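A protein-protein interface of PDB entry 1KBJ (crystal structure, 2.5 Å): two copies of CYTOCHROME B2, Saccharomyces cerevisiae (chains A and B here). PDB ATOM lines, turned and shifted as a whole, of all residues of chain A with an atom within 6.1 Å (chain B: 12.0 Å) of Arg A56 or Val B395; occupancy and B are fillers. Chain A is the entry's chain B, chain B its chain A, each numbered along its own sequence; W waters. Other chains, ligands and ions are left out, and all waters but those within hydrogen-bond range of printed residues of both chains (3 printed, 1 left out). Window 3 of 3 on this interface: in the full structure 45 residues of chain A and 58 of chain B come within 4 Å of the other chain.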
ATOM      1  N   ASP A  51       2.710   7.618  17.991  1.00  0.00           N
ATOM      2  CA  ASP A  51       2.742   7.570  16.534  1.00  0.00           C
ATOM      3  C   ASP A  51       2.951   8.936  15.854  1.00  0.00           C
ATOM      4  O   ASP A  51       3.028   9.026  14.644  1.00  0.00           O
ATOM      5  CB  ASP A  51       1.487   6.850  16.038  1.00  0.00           C
ATOM      6  CG  ASP A  51       1.457   5.376  16.498  1.00  0.00           C
ATOM      7  OD1 ASP A  51       0.391   4.878  16.949  1.00  0.00           O
ATOM      8  OD2 ASP A  51       2.510   4.707  16.413  1.00  0.00           O
ATOM      9  N   GLU A  52       3.079   9.992  16.653  1.00  0.00           N
ATOM     10  CA  GLU A  52       3.328  11.328  16.127  1.00  0.00           C
ATOM     11  C   GLU A  52       2.212  11.787  15.204  1.00  0.00           C
ATOM     12  O   GLU A  52       2.439  12.514  14.247  1.00  0.00           O
ATOM     13  CB  GLU A  52       4.675  11.349  15.373  1.00  0.00           C
ATOM     14  CG  GLU A  52       5.870  10.704  16.129  1.00  0.00           C
ATOM     15  CD  GLU A  52       7.253  11.067  15.541  1.00  0.00           C
ATOM     16  OE1 GLU A  52       7.373  11.208  14.301  1.00  0.00           O
ATOM     17  OE2 GLU A  52       8.220  11.196  16.326  1.00  0.00           O
ATOM     18  N   VAL A  53       0.992  11.381  15.493  1.00  0.00           N
ATOM     19  CA  VAL A  53      -0.113  11.770  14.632  1.00  0.00           C
ATOM     20  C   VAL A  53      -0.402  13.246  14.787  1.00  0.00           C
ATOM     21  O   VAL A  53      -0.490  13.972  13.783  1.00  0.00           O
ATOM     22  CB  VAL A  53      -1.366  10.950  14.949  1.00  0.00           C
ATOM     23  CG1 VAL A  53      -2.597  11.598  14.359  1.00  0.00           C
ATOM     24  CG2 VAL A  53      -1.210   9.578  14.384  1.00  0.00           C
ATOM     25  N   THR A  54      -0.542  13.690  16.040  1.00  0.00           N
ATOM     26  CA  THR A  54      -0.820  15.085  16.328  1.00  0.00           C
ATOM     27  C   THR A  54       0.315  16.003  15.852  1.00  0.00           C
ATOM     28  O   THR A  54       0.057  17.062  15.276  1.00  0.00           O
ATOM     29  CB  THR A  54      -1.088  15.315  17.834  1.00  0.00           C
ATOM     30  OG1 THR A  54      -2.370  14.781  18.177  1.00  0.00           O
ATOM     31  CG2 THR A  54      -1.111  16.801  18.144  1.00  0.00           C
ATOM     32  N   HIS A  55       1.563  15.599  16.062  1.00  0.00           N
ATOM     33  CA  HIS A  55       2.657  16.422  15.608  1.00  0.00           C
ATOM     34  C   HIS A  55       2.416  16.839  14.160  1.00  0.00           C
ATOM     35  O   HIS A  55       2.445  18.018  13.841  1.00  0.00           O
ATOM     36  CB  HIS A  55       3.958  15.664  15.732  1.00  0.00           C
ATOM     37  CG  HIS A  55       5.125  16.357  15.096  1.00  0.00           C
ATOM     38  ND1 HIS A  55       5.330  17.717  15.191  1.00  0.00           N
ATOM     39  CD2 HIS A  55       6.191  15.863  14.414  1.00  0.00           C
ATOM     40  CE1 HIS A  55       6.472  18.030  14.601  1.00  0.00           C
ATOM     41  NE2 HIS A  55       7.013  16.921  14.124  1.00  0.00           N
ATOM     42  N   ARG A  56       2.171  15.867  13.280  1.00  0.00           N
ATOM     43  CA  ARG A  56       1.913  16.164  11.869  1.00  0.00           C
ATOM     44  C   ARG A  56       0.567  16.878  11.684  1.00  0.00           C
ATOM     45  O   ARG A  56       0.475  17.867  10.952  1.00  0.00           O
ATOM     46  CB  ARG A  56       1.927  14.882  11.025  1.00  0.00           C
ATOM     47  CG  ARG A  56       3.320  14.304  10.749  1.00  0.00           C
ATOM     48  CD  ARG A  56       3.425  12.906  11.303  1.00  0.00           C
ATOM     49  NE  ARG A  56       3.000  11.913  10.340  1.00  0.00           N
ATOM     50  CZ  ARG A  56       2.500  10.714  10.633  1.00  0.00           C
ATOM     51  NH1 ARG A  56       2.323  10.310  11.886  1.00  0.00           N
ATOM     52  NH2 ARG A  56       2.221   9.894   9.641  1.00  0.00           N
ATOM     53  N   GLU A  57      -0.482  16.394  12.342  1.00  0.00           N
ATOM     54  CA  GLU A  57      -1.788  17.030  12.187  1.00  0.00           C
ATOM     55  C   GLU A  57      -1.741  18.536  12.519  1.00  0.00           C
ATOM     56  O   GLU A  57      -2.402  19.329  11.845  1.00  0.00           O
ATOM     57  CB  GLU A  57      -2.831  16.291  13.040  1.00  0.00           C
ATOM     58  CG  GLU A  57      -4.184  16.977  13.177  1.00  0.00           C
ATOM     59  CD  GLU A  57      -4.984  17.050  11.889  1.00  0.00           C
ATOM     60  OE1 GLU A  57      -4.613  16.386  10.901  1.00  0.00           O
ATOM     61  OE2 GLU A  57      -6.004  17.773  11.878  1.00  0.00           O
ATOM     62  N   ASN A  58      -0.951  18.935  13.523  1.00  0.00           N
ATOM     63  CA  ASN A  58      -0.842  20.345  13.883  1.00  0.00           C
ATOM     64  C   ASN A  58      -0.570  21.175  12.634  1.00  0.00           C
ATOM     65  O   ASN A  58      -1.139  22.248  12.459  1.00  0.00           O
ATOM     66  CB  ASN A  58       0.319  20.611  14.830  1.00  0.00           C
ATOM     67  CG  ASN A  58       0.121  20.040  16.231  1.00  0.00           C
ATOM     68  OD1 ASN A  58       1.109  19.821  16.929  1.00  0.00           O
ATOM     69  ND2 ASN A  58      -1.123  19.813  16.650  1.00  0.00           N
ATOM     70  N   HIS A  59       0.328  20.686  11.789  1.00  0.00           N
ATOM     71  CA  HIS A  59       0.700  21.369  10.559  1.00  0.00           C
ATOM     72  C   HIS A  59      -0.347  21.190   9.446  1.00  0.00           C
ATOM     73  O   HIS A  59      -0.816  22.157   8.856  1.00  0.00           O
ATOM     74  CB  HIS A  59       2.072  20.849  10.082  1.00  0.00           C
ATOM     75  CG  HIS A  59       2.475  21.356   8.731  1.00  0.00           C
ATOM     76  ND1 HIS A  59       2.745  22.684   8.484  1.00  0.00           N
ATOM     77  CD2 HIS A  59       2.538  20.732   7.531  1.00  0.00           C
ATOM     78  CE1 HIS A  59       2.941  22.859   7.189  1.00  0.00           C
ATOM     79  NE2 HIS A  59       2.820  21.689   6.589  1.00  0.00           N
ATOM     80  N   ASN A  60      -0.723  19.951   9.166  1.00  0.00           N
ATOM     81  CA  ASN A  60      -1.682  19.685   8.115  1.00  0.00           C
ATOM     82  C   ASN A  60      -3.033  20.394   8.237  1.00  0.00           C
ATOM     83  O   ASN A  60      -3.646  20.717   7.216  1.00  0.00           O
ATOM     84  CB  ASN A  60      -1.921  18.185   8.009  1.00  0.00           C
ATOM     85  CG  ASN A  60      -0.658  17.405   7.689  1.00  0.00           C
ATOM     86  OD1 ASN A  60      -0.595  16.202   7.918  1.00  0.00           O
ATOM     87  ND2 ASN A  60       0.345  18.081   7.155  1.00  0.00           N
ATOM     88  N   ALA A  61      -3.519  20.624   9.455  1.00  0.00           N
ATOM     89  CA  ALA A  61      -4.822  21.279   9.610  1.00  0.00           C
ATOM     90  C   ALA A  61      -4.812  22.678   9.000  1.00  0.00           C
ATOM     91  O   ALA A  61      -5.847  23.216   8.581  1.00  0.00           O
ATOM     92  CB  ALA A  61      -5.216  21.346  11.060  1.00  0.00           C
ATOM     93  N   PHE B 281      -2.587  29.004  -1.460  1.00  0.00           N
ATOM     94  CA  PHE B 281      -3.817  28.725  -0.734  1.00  0.00           C
ATOM     95  C   PHE B 281      -4.975  29.588  -1.176  1.00  0.00           C
ATOM     96  O   PHE B 281      -5.966  29.780  -0.460  1.00  0.00           O
ATOM     97  CB  PHE B 281      -3.635  28.753   0.781  1.00  0.00           C
ATOM     98  CG  PHE B 281      -3.090  27.464   1.310  1.00  0.00           C
ATOM     99  CD1 PHE B 281      -3.902  26.333   1.361  1.00  0.00           C
ATOM    100  CD2 PHE B 281      -1.726  27.333   1.607  1.00  0.00           C
ATOM    101  CE1 PHE B 281      -3.364  25.059   1.688  1.00  0.00           C
ATOM    102  CE2 PHE B 281      -1.181  26.086   1.929  1.00  0.00           C
ATOM    103  CZ  PHE B 281      -2.007  24.937   1.965  1.00  0.00           C
ATOM    104  N   VAL B 389      -8.011  16.690   3.720  1.00  0.00           N
ATOM    105  CA  VAL B 389      -6.657  16.575   4.237  1.00  0.00           C
ATOM    106  C   VAL B 389      -6.743  15.407   5.212  1.00  0.00           C
ATOM    107  O   VAL B 389      -7.353  15.495   6.299  1.00  0.00           O
ATOM    108  CB  VAL B 389      -6.182  17.846   4.985  1.00  0.00           C
ATOM    109  CG1 VAL B 389      -4.814  17.577   5.646  1.00  0.00           C
ATOM    110  CG2 VAL B 389      -6.070  19.010   4.015  1.00  0.00           C
ATOM    111  N   GLY B 390      -6.142  14.297   4.813  1.00  0.00           N
ATOM    112  CA  GLY B 390      -6.200  13.134   5.665  1.00  0.00           C
ATOM    113  C   GLY B 390      -5.399  13.212   6.951  1.00  0.00           C
ATOM    114  O   GLY B 390      -4.458  13.995   7.072  1.00  0.00           O
ATOM    115  N   VAL B 391      -5.821  12.406   7.921  1.00  0.00           N
ATOM    116  CA  VAL B 391      -5.145  12.265   9.186  1.00  0.00           C
ATOM    117  C   VAL B 391      -3.786  11.668   8.782  1.00  0.00           C
ATOM    118  O   VAL B 391      -3.709  10.845   7.870  1.00  0.00           O
ATOM    119  CB  VAL B 391      -5.952  11.295  10.092  1.00  0.00           C
ATOM    120  CG1 VAL B 391      -5.125  10.876  11.342  1.00  0.00           C
ATOM    121  CG2 VAL B 391      -7.244  11.975  10.500  1.00  0.00           C
ATOM    122  N   PRO B 392      -2.696  12.075   9.442  1.00  0.00           N
ATOM    123  CA  PRO B 392      -1.425  11.489   9.012  1.00  0.00           C
ATOM    124  C   PRO B 392      -1.333   9.973   9.122  1.00  0.00           C
ATOM    125  O   PRO B 392      -1.973   9.351   9.971  1.00  0.00           O
ATOM    126  CB  PRO B 392      -0.380  12.233   9.844  1.00  0.00           C
ATOM    127  CG  PRO B 392      -1.134  12.780  10.988  1.00  0.00           C
ATOM    128  CD  PRO B 392      -2.508  13.095  10.483  1.00  0.00           C
ATOM    129  N   ASN B 393      -0.541   9.395   8.227  1.00  0.00           N
ATOM    130  CA  ASN B 393      -0.314   7.963   8.161  1.00  0.00           C
ATOM    131  C   ASN B 393       0.240   7.303   9.393  1.00  0.00           C
ATOM    132  O   ASN B 393       1.181   7.808   9.986  1.00  0.00           O
ATOM    133  CB  ASN B 393       0.611   7.649   7.004  1.00  0.00           C
ATOM    134  CG  ASN B 393      -0.070   7.862   5.684  1.00  0.00           C
ATOM    135  OD1 ASN B 393      -1.237   7.466   5.514  1.00  0.00           O
ATOM    136  ND2 ASN B 393       0.630   8.501   4.738  1.00  0.00           N
ATOM    137  N   ASP B 394      -0.354   6.176   9.781  1.00  0.00           N
ATOM    138  CA  ASP B 394       0.131   5.420  10.931  1.00  0.00           C
ATOM    139  C   ASP B 394       1.308   4.644  10.318  1.00  0.00           C
ATOM    140  O   ASP B 394       1.135   3.521   9.861  1.00  0.00           O
ATOM    141  CB  ASP B 394      -0.975   4.471  11.424  1.00  0.00           C
ATOM    142  CG  ASP B 394      -0.616   3.779  12.714  1.00  0.00           C
ATOM    143  OD1 ASP B 394      -1.548   3.455  13.475  1.00  0.00           O
ATOM    144  OD2 ASP B 394       0.593   3.551  12.964  1.00  0.00           O
ATOM    145  N   VAL B 395       2.498   5.234  10.290  1.00  0.00           N
ATOM    146  CA  VAL B 395       3.594   4.551   9.645  1.00  0.00           C
ATOM    147  C   VAL B 395       3.940   3.175  10.183  1.00  0.00           C
ATOM    148  O   VAL B 395       4.115   2.262   9.388  1.00  0.00           O
ATOM    149  CB  VAL B 395       4.884   5.441   9.553  1.00  0.00           C
ATOM    150  CG1 VAL B 395       4.513   6.909   9.696  1.00  0.00           C
ATOM    151  CG2 VAL B 395       5.909   5.027  10.556  1.00  0.00           C
ATOM    152  N   LEU B 396       4.020   2.985  11.499  1.00  0.00           N
ATOM    153  CA  LEU B 396       4.361   1.654  12.006  1.00  0.00           C
ATOM    154  C   LEU B 396       3.319   0.623  11.569  1.00  0.00           C
ATOM    155  O   LEU B 396       3.666  -0.406  11.004  1.00  0.00           O
ATOM    156  CB  LEU B 396       4.493   1.656  13.531  1.00  0.00           C
ATOM    157  CG  LEU B 396       5.584   2.578  14.094  1.00  0.00           C
ATOM    158  CD1 LEU B 396       5.716   2.354  15.560  1.00  0.00           C
ATOM    159  CD2 LEU B 396       6.894   2.292  13.417  1.00  0.00           C
ATOM    160  N   TYR B 397       2.043   0.898  11.808  1.00  0.00           N
ATOM    161  CA  TYR B 397       0.990  -0.029  11.417  1.00  0.00           C
ATOM    162  C   TYR B 397       1.064  -0.445   9.930  1.00  0.00           C
ATOM    163  O   TYR B 397       0.954  -1.641   9.596  1.00  0.00           O
ATOM    164  CB  TYR B 397      -0.384   0.589  11.696  1.00  0.00           C
ATOM    165  CG  TYR B 397      -1.532  -0.353  11.385  1.00  0.00           C
ATOM    166  CD1 TYR B 397      -2.010  -1.232  12.350  1.00  0.00           C
ATOM    167  CD2 TYR B 397      -2.084  -0.413  10.097  1.00  0.00           C
ATOM    168  CE1 TYR B 397      -3.009  -2.151  12.051  1.00  0.00           C
ATOM    169  CE2 TYR B 397      -3.064  -1.319   9.785  1.00  0.00           C
ATOM    170  CZ  TYR B 397      -3.532  -2.190  10.771  1.00  0.00           C
ATOM    171  OH  TYR B 397      -4.530  -3.078  10.471  1.00  0.00           O
ATOM    172  N   ASN B 398       1.250   0.540   9.043  1.00  0.00           N
ATOM    173  CA  ASN B 398       1.319   0.284   7.610  1.00  0.00           C
ATOM    174  C   ASN B 398       2.648  -0.328   7.166  1.00  0.00           C
ATOM    175  O   ASN B 398       2.713  -1.103   6.201  1.00  0.00           O
ATOM    176  CB  ASN B 398       1.103   1.571   6.834  1.00  0.00           C
ATOM    177  CG  ASN B 398      -0.319   2.140   6.990  1.00  0.00           C
ATOM    178  OD1 ASN B 398      -0.557   3.311   6.682  1.00  0.00           O
ATOM    179  ND2 ASN B 398      -1.254   1.323   7.453  1.00  0.00           N
ATOM    180  N   GLU B 399       3.719   0.017   7.855  1.00  0.00           N
ATOM    181  CA  GLU B 399       4.997  -0.516   7.475  1.00  0.00           C
ATOM    182  C   GLU B 399       5.010  -2.018   7.746  1.00  0.00           C
ATOM    183  O   GLU B 399       5.364  -2.809   6.872  1.00  0.00           O
ATOM    184  CB  GLU B 399       6.106   0.181   8.259  1.00  0.00           C
ATOM    185  CG  GLU B 399       7.432  -0.533   8.177  1.00  0.00           C
ATOM    186  CD  GLU B 399       8.023  -0.503   6.776  1.00  0.00           C
ATOM    187  OE1 GLU B 399       8.782  -1.441   6.428  1.00  0.00           O
ATOM    188  OE2 GLU B 399       7.740   0.461   6.027  1.00  0.00           O
ATOM    189  N   VAL B 400       4.594  -2.410   8.949  1.00  0.00           N
ATOM    190  CA  VAL B 400       4.599  -3.812   9.333  1.00  0.00           C
ATOM    191  C   VAL B 400       3.562  -4.646   8.566  1.00  0.00           C
ATOM    192  O   VAL B 400       3.786  -5.814   8.277  1.00  0.00           O
ATOM    193  CB  VAL B 400       4.426  -3.954  10.888  1.00  0.00           C
ATOM    194  CG1 VAL B 400       2.956  -3.955  11.289  1.00  0.00           C
ATOM    195  CG2 VAL B 400       5.118  -5.185  11.359  1.00  0.00           C
ATOM    196  N   TYR B 401       2.433  -4.040   8.221  1.00  0.00           N
ATOM    197  CA  TYR B 401       1.391  -4.739   7.471  1.00  0.00           C
ATOM    198  C   TYR B 401       1.919  -5.264   6.143  1.00  0.00           C
ATOM    199  O   TYR B 401       2.721  -4.615   5.489  1.00  0.00           O
ATOM    200  CB  TYR B 401       0.212  -3.800   7.179  1.00  0.00           C
ATOM    201  CG  TYR B 401      -0.830  -4.432   6.280  1.00  0.00           C
ATOM    202  CD1 TYR B 401      -0.932  -4.087   4.931  1.00  0.00           C
ATOM    203  CD2 TYR B 401      -1.716  -5.397   6.781  1.00  0.00           C
ATOM    204  CE1 TYR B 401      -1.896  -4.685   4.111  1.00  0.00           C
ATOM    205  CE2 TYR B 401      -2.680  -6.000   5.969  1.00  0.00           C
ATOM    206  CZ  TYR B 401      -2.767  -5.639   4.650  1.00  0.00           C
ATOM    207  OH  TYR B 401      -3.767  -6.200   3.895  1.00  0.00           O
ATOM    208  N   GLU B 402       1.445  -6.436   5.750  1.00  0.00           N
ATOM    209  CA  GLU B 402       1.838  -7.069   4.489  1.00  0.00           C
ATOM    210  C   GLU B 402       0.568  -7.339   3.706  1.00  0.00           C
ATOM    211  O   GLU B 402      -0.236  -8.183   4.103  1.00  0.00           O
ATOM    212  CB  GLU B 402       2.521  -8.412   4.728  1.00  0.00           C
ATOM    213  CG  GLU B 402       3.989  -8.373   4.955  1.00  0.00           C
ATOM    214  CD  GLU B 402       4.517  -9.729   5.372  1.00  0.00           C
ATOM    215  OE1 GLU B 402       4.060 -10.749   4.813  1.00  0.00           O
ATOM    216  OE2 GLU B 402       5.390  -9.775   6.259  1.00  0.00           O
ATOM    217  N   GLY B 403       0.396  -6.640   2.589  1.00  0.00           N
ATOM    218  CA  GLY B 403      -0.801  -6.820   1.783  1.00  0.00           C
ATOM    219  C   GLY B 403      -0.883  -8.085   0.946  1.00  0.00           C
ATOM    220  O   GLY B 403       0.075  -8.843   0.843  1.00  0.00           O
HETATM  221  O   HOH W   1       2.985   7.037  12.537  1.00  0.00           O
HETATM  222  O   HOH W   2       2.803   4.415  13.457  1.00  0.00           O
HETATM  223  O   HOH W   3      -1.146   2.792  15.822  1.00  0.00           O
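Among the printed residues, merely in contact across the chains: Val A53 with Pro B392 (3.1 Å), Arg A56 with Pro B392 (3.4 Å), Asn A60 with Val B389 (3.7 Å), Arg A56 with Val B395 (3.8 Å) and Glu A57 with Pro B392 (3.9 Å).
Of the 11 printed residues of chain A, 4 touch a printed residue of chain B.
Hydrophobic or aromatic side chains of chain A within 4 Å of the printed part of chain B: Val A53.
Along chain A the printed residues that touch a printed residue of chain B span positions 53 to 60.
Of the 16 printed residues of chain B, 4 touch a printed residue of chain A.
Hydrophobic or aromatic side chains of chain B that line the printed part of chain A: Val B389, Pro B392 and Val B395.
Among the printed residues, 6 pairs touch across the chains.
Water W2 lies within hydrogen-bond range of the side-chain carboxylate of Asp B394 (2.4 Å), the backbone NH of Leu B396 (2.7 Å), the side-chain carboxylate of Asp A51 (3.0 Å) and the backbone NH of Val B395 (3.3 Å).
Water W3 bridges the side-chain carboxylate of Asp B394 (2.5 Å) and the side-chain carboxylate of Asp A51 (2.8 Å).
Water W1 lies within hydrogen-bond range of the backbone carbonyl oxygen of Asp A51, the backbone NH of Val B395, the backbone carbonyl oxygen of Asn B393 and the guanidinium group of Arg A56.
No residue of chain B comes within 4 Å of Asp A51.
No residue of chain B comes within 4 Å of His A55.
Of the printed residues of chain B, Glu A57 touches Pro B392.
No residue of chain B comes within 4 Å of Asn A58.
His A59 touches none of the printed residues of chain B.
Of chain B, only Val B389 comes within 4 Å of Asn A60.
Phe B281 touches none of the printed residues of chain A.
Of the printed residues of chain A, Val B389 touches Asn A60 (3.7 Å).
Gly B390 touches none of the printed residues of chain A.
Printed residues of chain A within 4 Å of Pro B392: Val A53 (3.1 Å), Arg A56 (3.4 Å) and Glu A57 (3.9 Å).
Of the printed residues of chain A, Asn B393 touches Arg A56 (2.4 Å).
The nearest residue of chain B that does not touch Arg A56 is Asp B394 (4.5 Å).
The nearest residue of chain A that does not touch Val B395 is Asp A51 (5.6 Å).
The nearest printed residue of chain A that does not touch Val B389 is Ala A61 (5.0 Å).
The backbone carbonyl oxygen (O) of Asn B393 sits close to the guanidinium group (NH1) of Arg A56, at 3.3 Å.
No position is printed for both chains.
O of Glu A52 sits close to NH1 of Arg A56, at 3.2 Å.
The guanidinium group (NH1) of Arg A56 lies within hydrogen-bond range of the backbone carbonyl oxygen (O) of Asp A51, 3.1 Å away.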
